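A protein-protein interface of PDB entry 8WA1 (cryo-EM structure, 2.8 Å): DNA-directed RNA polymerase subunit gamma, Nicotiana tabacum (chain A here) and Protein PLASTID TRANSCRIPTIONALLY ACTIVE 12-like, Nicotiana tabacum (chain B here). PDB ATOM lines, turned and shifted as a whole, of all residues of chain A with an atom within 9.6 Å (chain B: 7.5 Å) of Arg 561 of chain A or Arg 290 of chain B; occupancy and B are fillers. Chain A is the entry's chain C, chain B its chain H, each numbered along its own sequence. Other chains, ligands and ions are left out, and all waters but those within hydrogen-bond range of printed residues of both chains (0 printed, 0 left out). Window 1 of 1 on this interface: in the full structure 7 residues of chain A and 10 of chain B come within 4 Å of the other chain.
CD1 of Leu 293 of chain B touches O of Ile 557 of chain A (3.2 Å). Cys 558 of chain A touches Ala 289 of chain B (SG to O, 3.97 Å). Leu 293 of chain B touches Cys 558 of chain A. O of Val 559 of chain A touches CD2 of Leu 293 of chain B, at 3.3 Å. Leu 293 of chain B touches Asn 560 of chain A (CD1 to O, 3.6 Å). Arg 561 of chain A touches Leu 293 of chain B (N to CD1, 3.6 Å). Arg 561 of chain A touches Tyr 294 of chain B. Tyr 562 of chain A touches Leu 212 of chain B. Tyr 562 of chain A touches Gly 213 of chain B. Arg 214 of chain B touches Tyr 562 of chain A.
His 554 of chain A touches none of the printed residues of chain B. Arg 561 of chain A touches just these residues of chain B: Gly 213 (3.5 Å), Gln 271 (2.7 Å), Arg 290 (3.2 Å), Leu 293 (3.6 Å), Tyr 294 (3.4 Å) and Glu 297 (3.1 Å). Of the printed residues of chain B, Tyr 562 of chain A touches Leu 212, Gly 213 and Arg 214. Printed residues of chain B within 4 Å of Asn 563 of chain A: Leu 212 (3.5 Å). Printed residues of chain A within 4 Å of Leu 212 of chain B: Tyr 562 (3.2 Å) and Asn 563 (3.5 Å). Of the printed residues of chain A, Arg 214 of chain B touches Tyr 562 (3.9 Å). Ala 289 of chain B touches just one residue of chain A: Cys 558. Arg 290 of chain B touches just these residues of chain A: Ile 557 (3.3 Å), Asn 560 (3.2 Å) and Arg 561 (3.2 Å). Of the printed residues of chain A, Leu 293 of chain B touches Ile 557 (3.2 Å), Cys 558 (3.2 Å), Val 559 (3.3 Å), Asn 560 (3.6 Å) and Arg 561 (3.6 Å). Lys 295 of chain B touches none of the printed residues of chain A. The nearest residue of chain A that does not touch Arg 290 of chain B is Tyr 562 of chain A (4.9 Å).
Hydrophobic or aromatic side chains of chain B within 4 Å of the printed part of chain A: Leu 293 and Tyr 294. Along chain A the printed residues that touch a printed residue of chain B span positions 557 to 563. Among the printed residues, 17 pairs touch across the chains.
The side-chain hydroxyl (OH) of Tyr 562 of chain A is in hydrogen-bond range of the guanidinium group (NH2) of Arg 561 of chain A (3.4 Å). OD1 of Asn 563 of chain A lies within hydrogen-bond range of N of Cys 565 of chain A, 3.0 Å away. The guanidinium group of Arg 290 of chain B sits at hydrogen-bond distance from the side-chain hydroxyl of Tyr 294 of chain B, 3.0 Å away.
O of Ile 557 of chain A sits at hydrogen-bond distance from NH1 of Arg 290 of chain B (3.3 Å). The guanidinium group (NH1) of Arg 290 of chain B sits at hydrogen-bond distance from the backbone carbonyl oxygen (O) of Asn 560 of chain A, 3.2 Å away. The guanidinium group (NH1) of Arg 561 of chain A lies within hydrogen-bond range of the backbone carbonyl oxygen (O) of Gln 271 of chain B (2.7 Å). The backbone carbonyl oxygen (O) of Arg 561 of chain A sits at hydrogen-bond distance from the guanidinium group (NH1) of Arg 290 of chain B, at 3.2 Å. The guanidinium group (NH2) of Arg 561 of chain A lies within salt-bridge range of the side-chain carboxylate (OE1) of Glu 297 of chain B (3.1 Å).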
ATOM      1  N   HIS A 554       3.392 -31.012 -22.163  1.00  0.00           N
ATOM      2  CA  HIS A 554       2.424 -30.027 -22.621  1.00  0.00           C
ATOM      3  C   HIS A 554       2.590 -29.798 -24.117  1.00  0.00           C
ATOM      4  O   HIS A 554       3.656 -29.390 -24.585  1.00  0.00           O
ATOM      5  CB  HIS A 554       2.601 -28.716 -21.860  1.00  0.00           C
ATOM      6  CG  HIS A 554       2.336 -28.830 -20.393  1.00  0.00           C
ATOM      7  ND1 HIS A 554       2.970 -28.041 -19.458  1.00  0.00           N
ATOM      8  CD2 HIS A 554       1.505 -29.641 -19.698  1.00  0.00           C
ATOM      9  CE1 HIS A 554       2.542 -28.362 -18.249  1.00  0.00           C
ATOM     10  NE2 HIS A 554       1.651 -29.330 -18.368  1.00  0.00           N
ATOM     11  N   ARG A 555       1.529 -30.073 -24.870  1.00  0.00           N
ATOM     12  CA  ARG A 555       1.592 -30.091 -26.325  1.00  0.00           C
ATOM     13  C   ARG A 555       0.978 -28.847 -26.956  1.00  0.00           C
ATOM     14  O   ARG A 555       1.544 -28.293 -27.901  1.00  0.00           O
ATOM     15  CB  ARG A 555       0.906 -31.357 -26.856  1.00  0.00           C
ATOM     16  CG  ARG A 555       1.618 -32.644 -26.470  1.00  0.00           C
ATOM     17  CD  ARG A 555       0.787 -33.871 -26.805  1.00  0.00           C
ATOM     18  NE  ARG A 555       1.503 -35.107 -26.507  1.00  0.00           N
ATOM     19  CZ  ARG A 555       1.491 -35.712 -25.324  1.00  0.00           C
ATOM     20  NH1 ARG A 555       2.176 -36.833 -25.145  1.00  0.00           N
ATOM     21  NH2 ARG A 555       0.794 -35.197 -24.320  1.00  0.00           N
ATOM     22  N   GLY A 556      -0.169 -28.390 -26.462  1.00  0.00           N
ATOM     23  CA  GLY A 556      -0.879 -27.324 -27.141  1.00  0.00           C
ATOM     24  C   GLY A 556      -0.717 -25.945 -26.540  1.00  0.00           C
ATOM     25  O   GLY A 556       0.367 -25.358 -26.591  1.00  0.00           O
ATOM     26  N   ILE A 557      -1.797 -25.413 -25.967  1.00  0.00           N
ATOM     27  CA  ILE A 557      -1.772 -24.044 -25.457  1.00  0.00           C
ATOM     28  C   ILE A 557      -0.932 -23.957 -24.192  1.00  0.00           C
ATOM     29  O   ILE A 557      -0.505 -22.870 -23.788  1.00  0.00           O
ATOM     30  CB  ILE A 557      -3.206 -23.540 -25.218  1.00  0.00           C
ATOM     31  CG1 ILE A 557      -3.944 -24.476 -24.262  1.00  0.00           C
ATOM     32  CG2 ILE A 557      -3.948 -23.413 -26.533  1.00  0.00           C
ATOM     33  CD1 ILE A 557      -5.384 -24.092 -24.026  1.00  0.00           C
ATOM     34  N   CYS A 558      -0.689 -25.096 -23.542  1.00  0.00           N
ATOM     35  CA  CYS A 558       0.059 -25.085 -22.291  1.00  0.00           C
ATOM     36  C   CYS A 558       1.537 -24.798 -22.527  1.00  0.00           C
ATOM     37  O   CYS A 558       2.206 -24.210 -21.670  1.00  0.00           O
ATOM     38  CB  CYS A 558      -0.122 -26.417 -21.563  1.00  0.00           C
ATOM     39  SG  CYS A 558      -1.841 -26.837 -21.196  1.00  0.00           S
ATOM     40  N   VAL A 559       2.066 -25.206 -23.682  1.00  0.00           N
ATOM     41  CA  VAL A 559       3.500 -25.076 -23.921  1.00  0.00           C
ATOM     42  C   VAL A 559       3.829 -23.723 -24.547  1.00  0.00           C
ATOM     43  O   VAL A 559       4.936 -23.199 -24.372  1.00  0.00           O
ATOM     44  CB  VAL A 559       4.003 -26.245 -24.790  1.00  0.00           C
ATOM     45  CG1 VAL A 559       3.458 -26.147 -26.208  1.00  0.00           C
ATOM     46  CG2 VAL A 559       5.524 -26.302 -24.790  1.00  0.00           C
ATOM     47  N   ASN A 560       2.884 -23.132 -25.276  1.00  0.00           N
ATOM     48  CA  ASN A 560       3.109 -21.875 -25.975  1.00  0.00           C
ATOM     49  C   ASN A 560       1.958 -20.918 -25.707  1.00  0.00           C
ATOM     50  O   ASN A 560       0.792 -21.326 -25.689  1.00  0.00           O
ATOM     51  CB  ASN A 560       3.260 -22.096 -27.485  1.00  0.00           C
ATOM     52  CG  ASN A 560       4.467 -22.941 -27.832  1.00  0.00           C
ATOM     53  OD1 ASN A 560       5.499 -22.876 -27.163  1.00  0.00           O
ATOM     54  ND2 ASN A 560       4.345 -23.741 -28.885  1.00  0.00           N
ATOM     55  N   ARG A 561       2.288 -19.641 -25.509  1.00  0.00           N
ATOM     56  CA  ARG A 561       1.261 -18.639 -25.263  1.00  0.00           C
ATOM     57  C   ARG A 561       0.638 -18.105 -26.545  1.00  0.00           C
ATOM     58  O   ARG A 561      -0.558 -17.794 -26.555  1.00  0.00           O
ATOM     59  CB  ARG A 561       1.836 -17.475 -24.454  1.00  0.00           C
ATOM     60  CG  ARG A 561       0.785 -16.471 -24.012  1.00  0.00           C
ATOM     61  CD  ARG A 561       1.405 -15.231 -23.406  1.00  0.00           C
ATOM     62  NE  ARG A 561       0.389 -14.244 -23.056  1.00  0.00           N
ATOM     63  CZ  ARG A 561       0.653 -13.054 -22.528  1.00  0.00           C
ATOM     64  NH1 ARG A 561      -0.336 -12.220 -22.241  1.00  0.00           N
ATOM     65  NH2 ARG A 561       1.907 -12.696 -22.287  1.00  0.00           N
ATOM     66  N   TYR A 562       1.408 -18.014 -27.626  1.00  0.00           N
ATOM     67  CA  TYR A 562       0.905 -17.514 -28.895  1.00  0.00           C
ATOM     68  C   TYR A 562       0.999 -18.621 -29.932  1.00  0.00           C
ATOM     69  O   TYR A 562       1.742 -19.593 -29.767  1.00  0.00           O
ATOM     70  CB  TYR A 562       1.679 -16.275 -29.366  1.00  0.00           C
ATOM     71  CG  TYR A 562       1.675 -15.134 -28.374  1.00  0.00           C
ATOM     72  CD1 TYR A 562       0.633 -14.219 -28.342  1.00  0.00           C
ATOM     73  CD2 TYR A 562       2.716 -14.973 -27.469  1.00  0.00           C
ATOM     74  CE1 TYR A 562       0.625 -13.175 -27.436  1.00  0.00           C
ATOM     75  CE2 TYR A 562       2.717 -13.932 -26.561  1.00  0.00           C
ATOM     76  CZ  TYR A 562       1.670 -13.037 -26.549  1.00  0.00           C
ATOM     77  OH  TYR A 562       1.666 -11.999 -25.646  1.00  0.00           O
ATOM     78  N   ASN A 563       0.230 -18.463 -31.001  1.00  0.00           N
ATOM     79  CA  ASN A 563       0.225 -19.457 -32.063  1.00  0.00           C
ATOM     80  C   ASN A 563       1.587 -19.482 -32.753  1.00  0.00           C
ATOM     81  O   ASN A 563       2.102 -18.431 -33.153  1.00  0.00           O
ATOM     82  CB  ASN A 563      -0.878 -19.139 -33.076  1.00  0.00           C
ATOM     83  CG  ASN A 563      -1.195 -20.309 -33.994  1.00  0.00           C
ATOM     84  OD1 ASN A 563      -0.308 -21.058 -34.403  1.00  0.00           O
ATOM     85  ND2 ASN A 563      -2.470 -20.463 -34.329  1.00  0.00           N
ATOM     86  N   PRO A 564       2.203 -20.659 -32.906  1.00  0.00           N
ATOM     87  CA  PRO A 564       3.483 -20.734 -33.627  1.00  0.00           C
ATOM     88  C   PRO A 564       3.383 -20.398 -35.108  1.00  0.00           C
ATOM     89  O   PRO A 564       4.408 -20.447 -35.800  1.00  0.00           O
ATOM     90  CB  PRO A 564       3.917 -22.194 -33.424  1.00  0.00           C
ATOM     91  CG  PRO A 564       3.175 -22.647 -32.206  1.00  0.00           C
ATOM     92  CD  PRO A 564       1.858 -21.936 -32.258  1.00  0.00           C
ATOM     93  N   CYS A 565       2.193 -20.065 -35.615  1.00  0.00           N
ATOM     94  CA  CYS A 565       2.056 -19.718 -37.026  1.00  0.00           C
ATOM     95  C   CYS A 565       2.865 -18.475 -37.373  1.00  0.00           C
ATOM     96  O   CYS A 565       3.465 -18.396 -38.452  1.00  0.00           O
ATOM     97  CB  CYS A 565       0.583 -19.510 -37.377  1.00  0.00           C
ATOM     98  SG  CYS A 565       0.284 -19.017 -39.091  1.00  0.00           S
ATOM     99  N   ASN A 566       2.891 -17.490 -36.472  1.00  0.00           N
ATOM    100  CA  ASN A 566       3.646 -16.269 -36.733  1.00  0.00           C
ATOM    101  C   ASN A 566       5.141 -16.552 -36.822  1.00  0.00           C
ATOM    102  O   ASN A 566       5.864 -15.889 -37.577  1.00  0.00           O
ATOM    103  CB  ASN A 566       3.360 -15.231 -35.648  1.00  0.00           C
ATOM    104  CG  ASN A 566       3.694 -15.733 -34.258  1.00  0.00           C
ATOM    105  OD1 ASN A 566       4.855 -15.741 -33.848  1.00  0.00           O
ATOM    106  ND2 ASN A 566       2.673 -16.153 -33.519  1.00  0.00           N
ATOM    107  N   LEU B 212      -3.561 -15.142 -33.427  1.00  0.00           N
ATOM    108  CA  LEU B 212      -2.268 -15.031 -32.764  1.00  0.00           C
ATOM    109  C   LEU B 212      -2.327 -15.376 -31.282  1.00  0.00           C
ATOM    110  O   LEU B 212      -1.299 -15.298 -30.601  1.00  0.00           O
ATOM    111  CB  LEU B 212      -1.703 -13.619 -32.941  1.00  0.00           C
ATOM    112  CG  LEU B 212      -1.423 -13.157 -34.370  1.00  0.00           C
ATOM    113  CD1 LEU B 212      -0.825 -11.760 -34.369  1.00  0.00           C
ATOM    114  CD2 LEU B 212      -0.504 -14.137 -35.083  1.00  0.00           C
ATOM    115  N   GLY B 213      -3.493 -15.757 -30.769  1.00  0.00           N
ATOM    116  CA  GLY B 213      -3.625 -16.105 -29.368  1.00  0.00           C
ATOM    117  C   GLY B 213      -3.366 -14.945 -28.427  1.00  0.00           C
ATOM    118  O   GLY B 213      -2.647 -15.089 -27.434  1.00  0.00           O
ATOM    119  N   ARG B 214      -3.950 -13.790 -28.732  1.00  0.00           N
ATOM    120  CA  ARG B 214      -3.795 -12.588 -27.923  1.00  0.00           C
ATOM    121  C   ARG B 214      -5.050 -12.378 -27.083  1.00  0.00           C
ATOM    122  O   ARG B 214      -6.095 -12.971 -27.381  1.00  0.00           O
ATOM    123  CB  ARG B 214      -3.517 -11.382 -28.826  1.00  0.00           C
ATOM    124  CG  ARG B 214      -2.131 -11.395 -29.455  1.00  0.00           C
ATOM    125  CD  ARG B 214      -2.042 -10.460 -30.652  1.00  0.00           C
ATOM    126  NE  ARG B 214      -2.424  -9.092 -30.318  1.00  0.00           N
ATOM    127  CZ  ARG B 214      -2.399  -8.081 -31.180  1.00  0.00           C
ATOM    128  NH1 ARG B 214      -2.007  -8.284 -32.430  1.00  0.00           N
ATOM    129  NH2 ARG B 214      -2.766  -6.867 -30.793  1.00  0.00           N
ATOM    130  N   PRO B 215      -4.992 -11.567 -26.025  1.00  0.00           N
ATOM    131  CA  PRO B 215      -6.190 -11.348 -25.196  1.00  0.00           C
ATOM    132  C   PRO B 215      -7.338 -10.768 -26.007  1.00  0.00           C
ATOM    133  O   PRO B 215      -7.238  -9.676 -26.569  1.00  0.00           O
ATOM    134  CB  PRO B 215      -5.698 -10.369 -24.124  1.00  0.00           C
ATOM    135  CG  PRO B 215      -4.239 -10.639 -24.024  1.00  0.00           C
ATOM    136  CD  PRO B 215      -3.791 -10.965 -25.419  1.00  0.00           C
ATOM    137  N   MET B 266      -1.791  -9.978 -12.082  1.00  0.00           N
ATOM    138  CA  MET B 266      -1.232  -9.860 -13.423  1.00  0.00           C
ATOM    139  C   MET B 266      -2.121  -9.076 -14.380  1.00  0.00           C
ATOM    140  O   MET B 266      -1.664  -8.724 -15.472  1.00  0.00           O
ATOM    141  CB  MET B 266      -0.947 -11.245 -14.011  1.00  0.00           C
ATOM    142  CG  MET B 266      -2.179 -12.081 -14.288  1.00  0.00           C
ATOM    143  SD  MET B 266      -1.739 -13.676 -14.997  1.00  0.00           S
ATOM    144  CE  MET B 266      -0.464 -14.191 -13.853  1.00  0.00           C
ATOM    145  N   GLY B 270      -0.269  -4.905 -17.257  1.00  0.00           N
ATOM    146  CA  GLY B 270      -0.525  -5.171 -18.658  1.00  0.00           C
ATOM    147  C   GLY B 270      -0.099  -6.530 -19.165  1.00  0.00           C
ATOM    148  O   GLY B 270       0.025  -6.701 -20.384  1.00  0.00           O
ATOM    149  N   GLN B 271       0.131  -7.504 -18.282  1.00  0.00           N
ATOM    150  CA  GLN B 271       0.530  -8.829 -18.747  1.00  0.00           C
ATOM    151  C   GLN B 271      -0.632  -9.548 -19.422  1.00  0.00           C
ATOM    152  O   GLN B 271      -0.452 -10.194 -20.460  1.00  0.00           O
ATOM    153  CB  GLN B 271       1.075  -9.655 -17.583  1.00  0.00           C
ATOM    154  CG  GLN B 271       1.756 -10.947 -18.011  1.00  0.00           C
ATOM    155  CD  GLN B 271       2.403 -11.680 -16.852  1.00  0.00           C
ATOM    156  OE1 GLN B 271       2.879 -12.805 -17.003  1.00  0.00           O
ATOM    157  NE2 GLN B 271       2.426 -11.043 -15.687  1.00  0.00           N
ATOM    158  N   VAL B 272      -1.830  -9.452 -18.844  1.00  0.00           N
ATOM    159  CA  VAL B 272      -3.031 -10.045 -19.415  1.00  0.00           C
ATOM    160  C   VAL B 272      -4.155  -9.022 -19.352  1.00  0.00           C
ATOM    161  O   VAL B 272      -4.061  -7.997 -18.675  1.00  0.00           O
ATOM    162  CB  VAL B 272      -3.457 -11.344 -18.694  1.00  0.00           C
ATOM    163  CG1 VAL B 272      -2.329 -12.369 -18.710  1.00  0.00           C
ATOM    164  CG2 VAL B 272      -3.896 -11.040 -17.273  1.00  0.00           C
ATOM    165  N   LYS B 273      -5.233  -9.318 -20.074  1.00  0.00           N
ATOM    166  CA  LYS B 273      -6.427  -8.483 -20.086  1.00  0.00           C
ATOM    167  C   LYS B 273      -7.644  -9.358 -19.835  1.00  0.00           C
ATOM    168  O   LYS B 273      -7.807 -10.400 -20.480  1.00  0.00           O
ATOM    169  CB  LYS B 273      -6.574  -7.733 -21.414  1.00  0.00           C
ATOM    170  CG  LYS B 273      -5.470  -6.727 -21.684  1.00  0.00           C
ATOM    171  CD  LYS B 273      -5.707  -5.983 -22.986  1.00  0.00           C
ATOM    172  CE  LYS B 273      -4.615  -4.959 -23.241  1.00  0.00           C
ATOM    173  NZ  LYS B 273      -4.531  -3.959 -22.142  1.00  0.00           N
ATOM    174  N   THR B 284     -10.349 -18.047 -14.450  1.00  0.00           N
ATOM    175  CA  THR B 284      -9.568 -18.741 -13.430  1.00  0.00           C
ATOM    176  C   THR B 284      -9.174 -20.137 -13.895  1.00  0.00           C
ATOM    177  O   THR B 284      -8.053 -20.587 -13.636  1.00  0.00           O
ATOM    178  CB  THR B 284     -10.344 -18.816 -12.115  1.00  0.00           C
ATOM    179  OG1 THR B 284     -11.558 -19.550 -12.310  1.00  0.00           O
ATOM    180  CG2 THR B 284     -10.668 -17.420 -11.605  1.00  0.00           C
ATOM    181  N   ALA B 285     -10.074 -20.832 -14.595  1.00  0.00           N
ATOM    182  CA  ALA B 285      -9.727 -22.143 -15.138  1.00  0.00           C
ATOM    183  C   ALA B 285      -8.659 -22.026 -16.221  1.00  0.00           C
ATOM    184  O   ALA B 285      -7.717 -22.830 -16.270  1.00  0.00           O
ATOM    185  CB  ALA B 285     -10.976 -22.834 -15.683  1.00  0.00           C
ATOM    186  N   LEU B 286      -8.784 -21.025 -17.095  1.00  0.00           N
ATOM    187  CA  LEU B 286      -7.773 -20.810 -18.126  1.00  0.00           C
ATOM    188  C   LEU B 286      -6.413 -20.509 -17.506  1.00  0.00           C
ATOM    189  O   LEU B 286      -5.377 -20.973 -17.999  1.00  0.00           O
ATOM    190  CB  LEU B 286      -8.207 -19.676 -19.052  1.00  0.00           C
ATOM    191  CG  LEU B 286      -7.438 -19.515 -20.362  1.00  0.00           C
ATOM    192  CD1 LEU B 286      -7.645 -20.731 -21.252  1.00  0.00           C
ATOM    193  CD2 LEU B 286      -7.865 -18.244 -21.078  1.00  0.00           C
ATOM    194  N   TYR B 287      -6.398 -19.740 -16.415  1.00  0.00           N
ATOM    195  CA  TYR B 287      -5.140 -19.464 -15.731  1.00  0.00           C
ATOM    196  C   TYR B 287      -4.587 -20.718 -15.067  1.00  0.00           C
ATOM    197  O   TYR B 287      -3.379 -20.970 -15.111  1.00  0.00           O
ATOM    198  CB  TYR B 287      -5.327 -18.354 -14.699  1.00  0.00           C
ATOM    199  CG  TYR B 287      -4.112 -18.159 -13.827  1.00  0.00           C
ATOM    200  CD1 TYR B 287      -2.980 -17.524 -14.316  1.00  0.00           C
ATOM    201  CD2 TYR B 287      -4.090 -18.624 -12.519  1.00  0.00           C
ATOM    202  CE1 TYR B 287      -1.865 -17.351 -13.526  1.00  0.00           C
ATOM    203  CE2 TYR B 287      -2.978 -18.455 -11.722  1.00  0.00           C
ATOM    204  CZ  TYR B 287      -1.868 -17.817 -12.231  1.00  0.00           C
ATOM    205  OH  TYR B 287      -0.757 -17.646 -11.441  1.00  0.00           O
ATOM    206  N   ARG B 288      -5.455 -21.514 -14.439  1.00  0.00           N
ATOM    207  CA  ARG B 288      -5.020 -22.788 -13.876  1.00  0.00           C
ATOM    208  C   ARG B 288      -4.378 -23.657 -14.949  1.00  0.00           C
ATOM    209  O   ARG B 288      -3.450 -24.427 -14.675  1.00  0.00           O
ATOM    210  CB  ARG B 288      -6.210 -23.508 -13.241  1.00  0.00           C
ATOM    211  CG  ARG B 288      -5.853 -24.785 -12.500  1.00  0.00           C
ATOM    212  CD  ARG B 288      -7.106 -25.562 -12.139  1.00  0.00           C
ATOM    213  NE  ARG B 288      -8.108 -24.711 -11.504  1.00  0.00           N
ATOM    214  CZ  ARG B 288      -9.361 -25.083 -11.261  1.00  0.00           C
ATOM    215  NH1 ARG B 288      -9.773 -26.295 -11.603  1.00  0.00           N
ATOM    216  NH2 ARG B 288     -10.203 -24.240 -10.680  1.00  0.00           N
ATOM    217  N   ALA B 289      -4.864 -23.540 -16.184  1.00  0.00           N
ATOM    218  CA  ALA B 289      -4.291 -24.319 -17.276  1.00  0.00           C
ATOM    219  C   ALA B 289      -2.950 -23.750 -17.736  1.00  0.00           C
ATOM    220  O   ALA B 289      -2.008 -24.510 -17.989  1.00  0.00           O
ATOM    221  CB  ALA B 289      -5.277 -24.386 -18.441  1.00  0.00           C
ATOM    222  N   ARG B 290      -2.840 -22.424 -17.851  1.00  0.00           N
ATOM    223  CA  ARG B 290      -1.722 -21.808 -18.561  1.00  0.00           C
ATOM    224  C   ARG B 290      -0.831 -20.931 -17.674  1.00  0.00           C
ATOM    225  O   ARG B 290      -0.146 -20.043 -18.193  1.00  0.00           O
ATOM    226  CB  ARG B 290      -2.252 -20.990 -19.738  1.00  0.00           C
ATOM    227  CG  ARG B 290      -3.343 -21.700 -20.523  1.00  0.00           C
ATOM    228  CD  ARG B 290      -3.956 -20.808 -21.589  1.00  0.00           C
ATOM    229  NE  ARG B 290      -3.144 -20.747 -22.800  1.00  0.00           N
ATOM    230  CZ  ARG B 290      -2.346 -19.734 -23.116  1.00  0.00           C
ATOM    231  NH1 ARG B 290      -1.647 -19.769 -24.242  1.00  0.00           N
ATOM    232  NH2 ARG B 290      -2.251 -18.683 -22.314  1.00  0.00           N
ATOM    233  N   ARG B 291      -0.813 -21.162 -16.359  1.00  0.00           N
ATOM    234  CA  ARG B 291      -0.020 -20.312 -15.471  1.00  0.00           C
ATOM    235  C   ARG B 291       1.479 -20.488 -15.693  1.00  0.00           C
ATOM    236  O   ARG B 291       2.267 -19.575 -15.402  1.00  0.00           O
ATOM    237  CB  ARG B 291      -0.385 -20.607 -14.014  1.00  0.00           C
ATOM    238  CG  ARG B 291       0.687 -21.347 -13.227  1.00  0.00           C
ATOM    239  CD  ARG B 291       0.093 -22.099 -12.050  1.00  0.00           C
ATOM    240  NE  ARG B 291      -0.775 -23.190 -12.485  1.00  0.00           N
ATOM    241  CZ  ARG B 291      -1.347 -24.061 -11.661  1.00  0.00           C
ATOM    242  NH1 ARG B 291      -1.144 -23.969 -10.354  1.00  0.00           N
ATOM    243  NH2 ARG B 291      -2.122 -25.024 -12.142  1.00  0.00           N
ATOM    244  N   HIS B 292       1.895 -21.657 -16.190  1.00  0.00           N
ATOM    245  CA  HIS B 292       3.321 -21.927 -16.346  1.00  0.00           C
ATOM    246  C   HIS B 292       3.957 -20.973 -17.348  1.00  0.00           C
ATOM    247  O   HIS B 292       5.104 -20.543 -17.169  1.00  0.00           O
ATOM    248  CB  HIS B 292       3.536 -23.378 -16.778  1.00  0.00           C
ATOM    249  CG  HIS B 292       2.706 -24.364 -16.015  1.00  0.00           C
ATOM    250  ND1 HIS B 292       1.386 -24.619 -16.320  1.00  0.00           N
ATOM    251  CD2 HIS B 292       3.007 -25.156 -14.959  1.00  0.00           C
ATOM    252  CE1 HIS B 292       0.911 -25.526 -15.485  1.00  0.00           C
ATOM    253  NE2 HIS B 292       1.874 -25.869 -14.650  1.00  0.00           N
ATOM    254  N   LEU B 293       3.222 -20.623 -18.405  1.00  0.00           N
ATOM    255  CA  LEU B 293       3.742 -19.697 -19.404  1.00  0.00           C
ATOM    256  C   LEU B 293       4.053 -18.339 -18.791  1.00  0.00           C
ATOM    257  O   LEU B 293       5.138 -17.787 -19.004  1.00  0.00           O
ATOM    258  CB  LEU B 293       2.739 -19.551 -20.546  1.00  0.00           C
ATOM    259  CG  LEU B 293       2.389 -20.854 -21.256  1.00  0.00           C
ATOM    260  CD1 LEU B 293       1.222 -20.652 -22.203  1.00  0.00           C
ATOM    261  CD2 LEU B 293       3.606 -21.370 -22.000  1.00  0.00           C
ATOM    262  N   TYR B 294       3.113 -17.787 -18.025  1.00  0.00           N
ATOM    263  CA  TYR B 294       3.330 -16.477 -17.421  1.00  0.00           C
ATOM    264  C   TYR B 294       4.413 -16.534 -16.351  1.00  0.00           C
ATOM    265  O   TYR B 294       5.186 -15.581 -16.191  1.00  0.00           O
ATOM    266  CB  TYR B 294       2.017 -15.946 -16.848  1.00  0.00           C
ATOM    267  CG  TYR B 294       0.872 -16.030 -17.828  1.00  0.00           C
ATOM    268  CD1 TYR B 294       0.801 -15.173 -18.918  1.00  0.00           C
ATOM    269  CD2 TYR B 294      -0.132 -16.975 -17.672  1.00  0.00           C
ATOM    270  CE1 TYR B 294      -0.242 -15.251 -19.820  1.00  0.00           C
ATOM    271  CE2 TYR B 294      -1.178 -17.060 -18.568  1.00  0.00           C
ATOM    272  CZ  TYR B 294      -1.228 -16.196 -19.640  1.00  0.00           C
ATOM    273  OH  TYR B 294      -2.269 -16.280 -20.534  1.00  0.00           O
ATOM    274  N   LYS B 295       4.496 -17.648 -15.618  1.00  0.00           N
ATOM    275  CA  LYS B 295       5.574 -17.800 -14.645  1.00  0.00           C
ATOM    276  C   LYS B 295       6.934 -17.781 -15.331  1.00  0.00           C
ATOM    277  O   LYS B 295       7.859 -17.088 -14.886  1.00  0.00           O
ATOM    278  CB  LYS B 295       5.387 -19.091 -13.851  1.00  0.00           C
ATOM    279  CG  LYS B 295       6.423 -19.312 -12.763  1.00  0.00           C
ATOM    280  CD  LYS B 295       6.292 -20.696 -12.145  1.00  0.00           C
ATOM    281  CE  LYS B 295       4.921 -20.900 -11.519  1.00  0.00           C
ATOM    282  NZ  LYS B 295       4.787 -22.245 -10.892  1.00  0.00           N
ATOM    283  N   GLU B 297       7.604 -16.477 -18.239  1.00  0.00           N
ATOM    284  CA  GLU B 297       7.825 -15.151 -18.808  1.00  0.00           C
ATOM    285  C   GLU B 297       8.324 -14.173 -17.753  1.00  0.00           C
ATOM    286  O   GLU B 297       9.239 -13.381 -18.013  1.00  0.00           O
ATOM    287  CB  GLU B 297       6.543 -14.636 -19.459  1.00  0.00           C
ATOM    288  CG  GLU B 297       6.182 -15.350 -20.750  1.00  0.00           C
ATOM    289  CD  GLU B 297       4.892 -14.838 -21.357  1.00  0.00           C
ATOM    290  OE1 GLU B 297       4.359 -13.827 -20.855  1.00  0.00           O
ATOM    291  OE2 GLU B 297       4.413 -15.447 -22.335  1.00  0.00           O
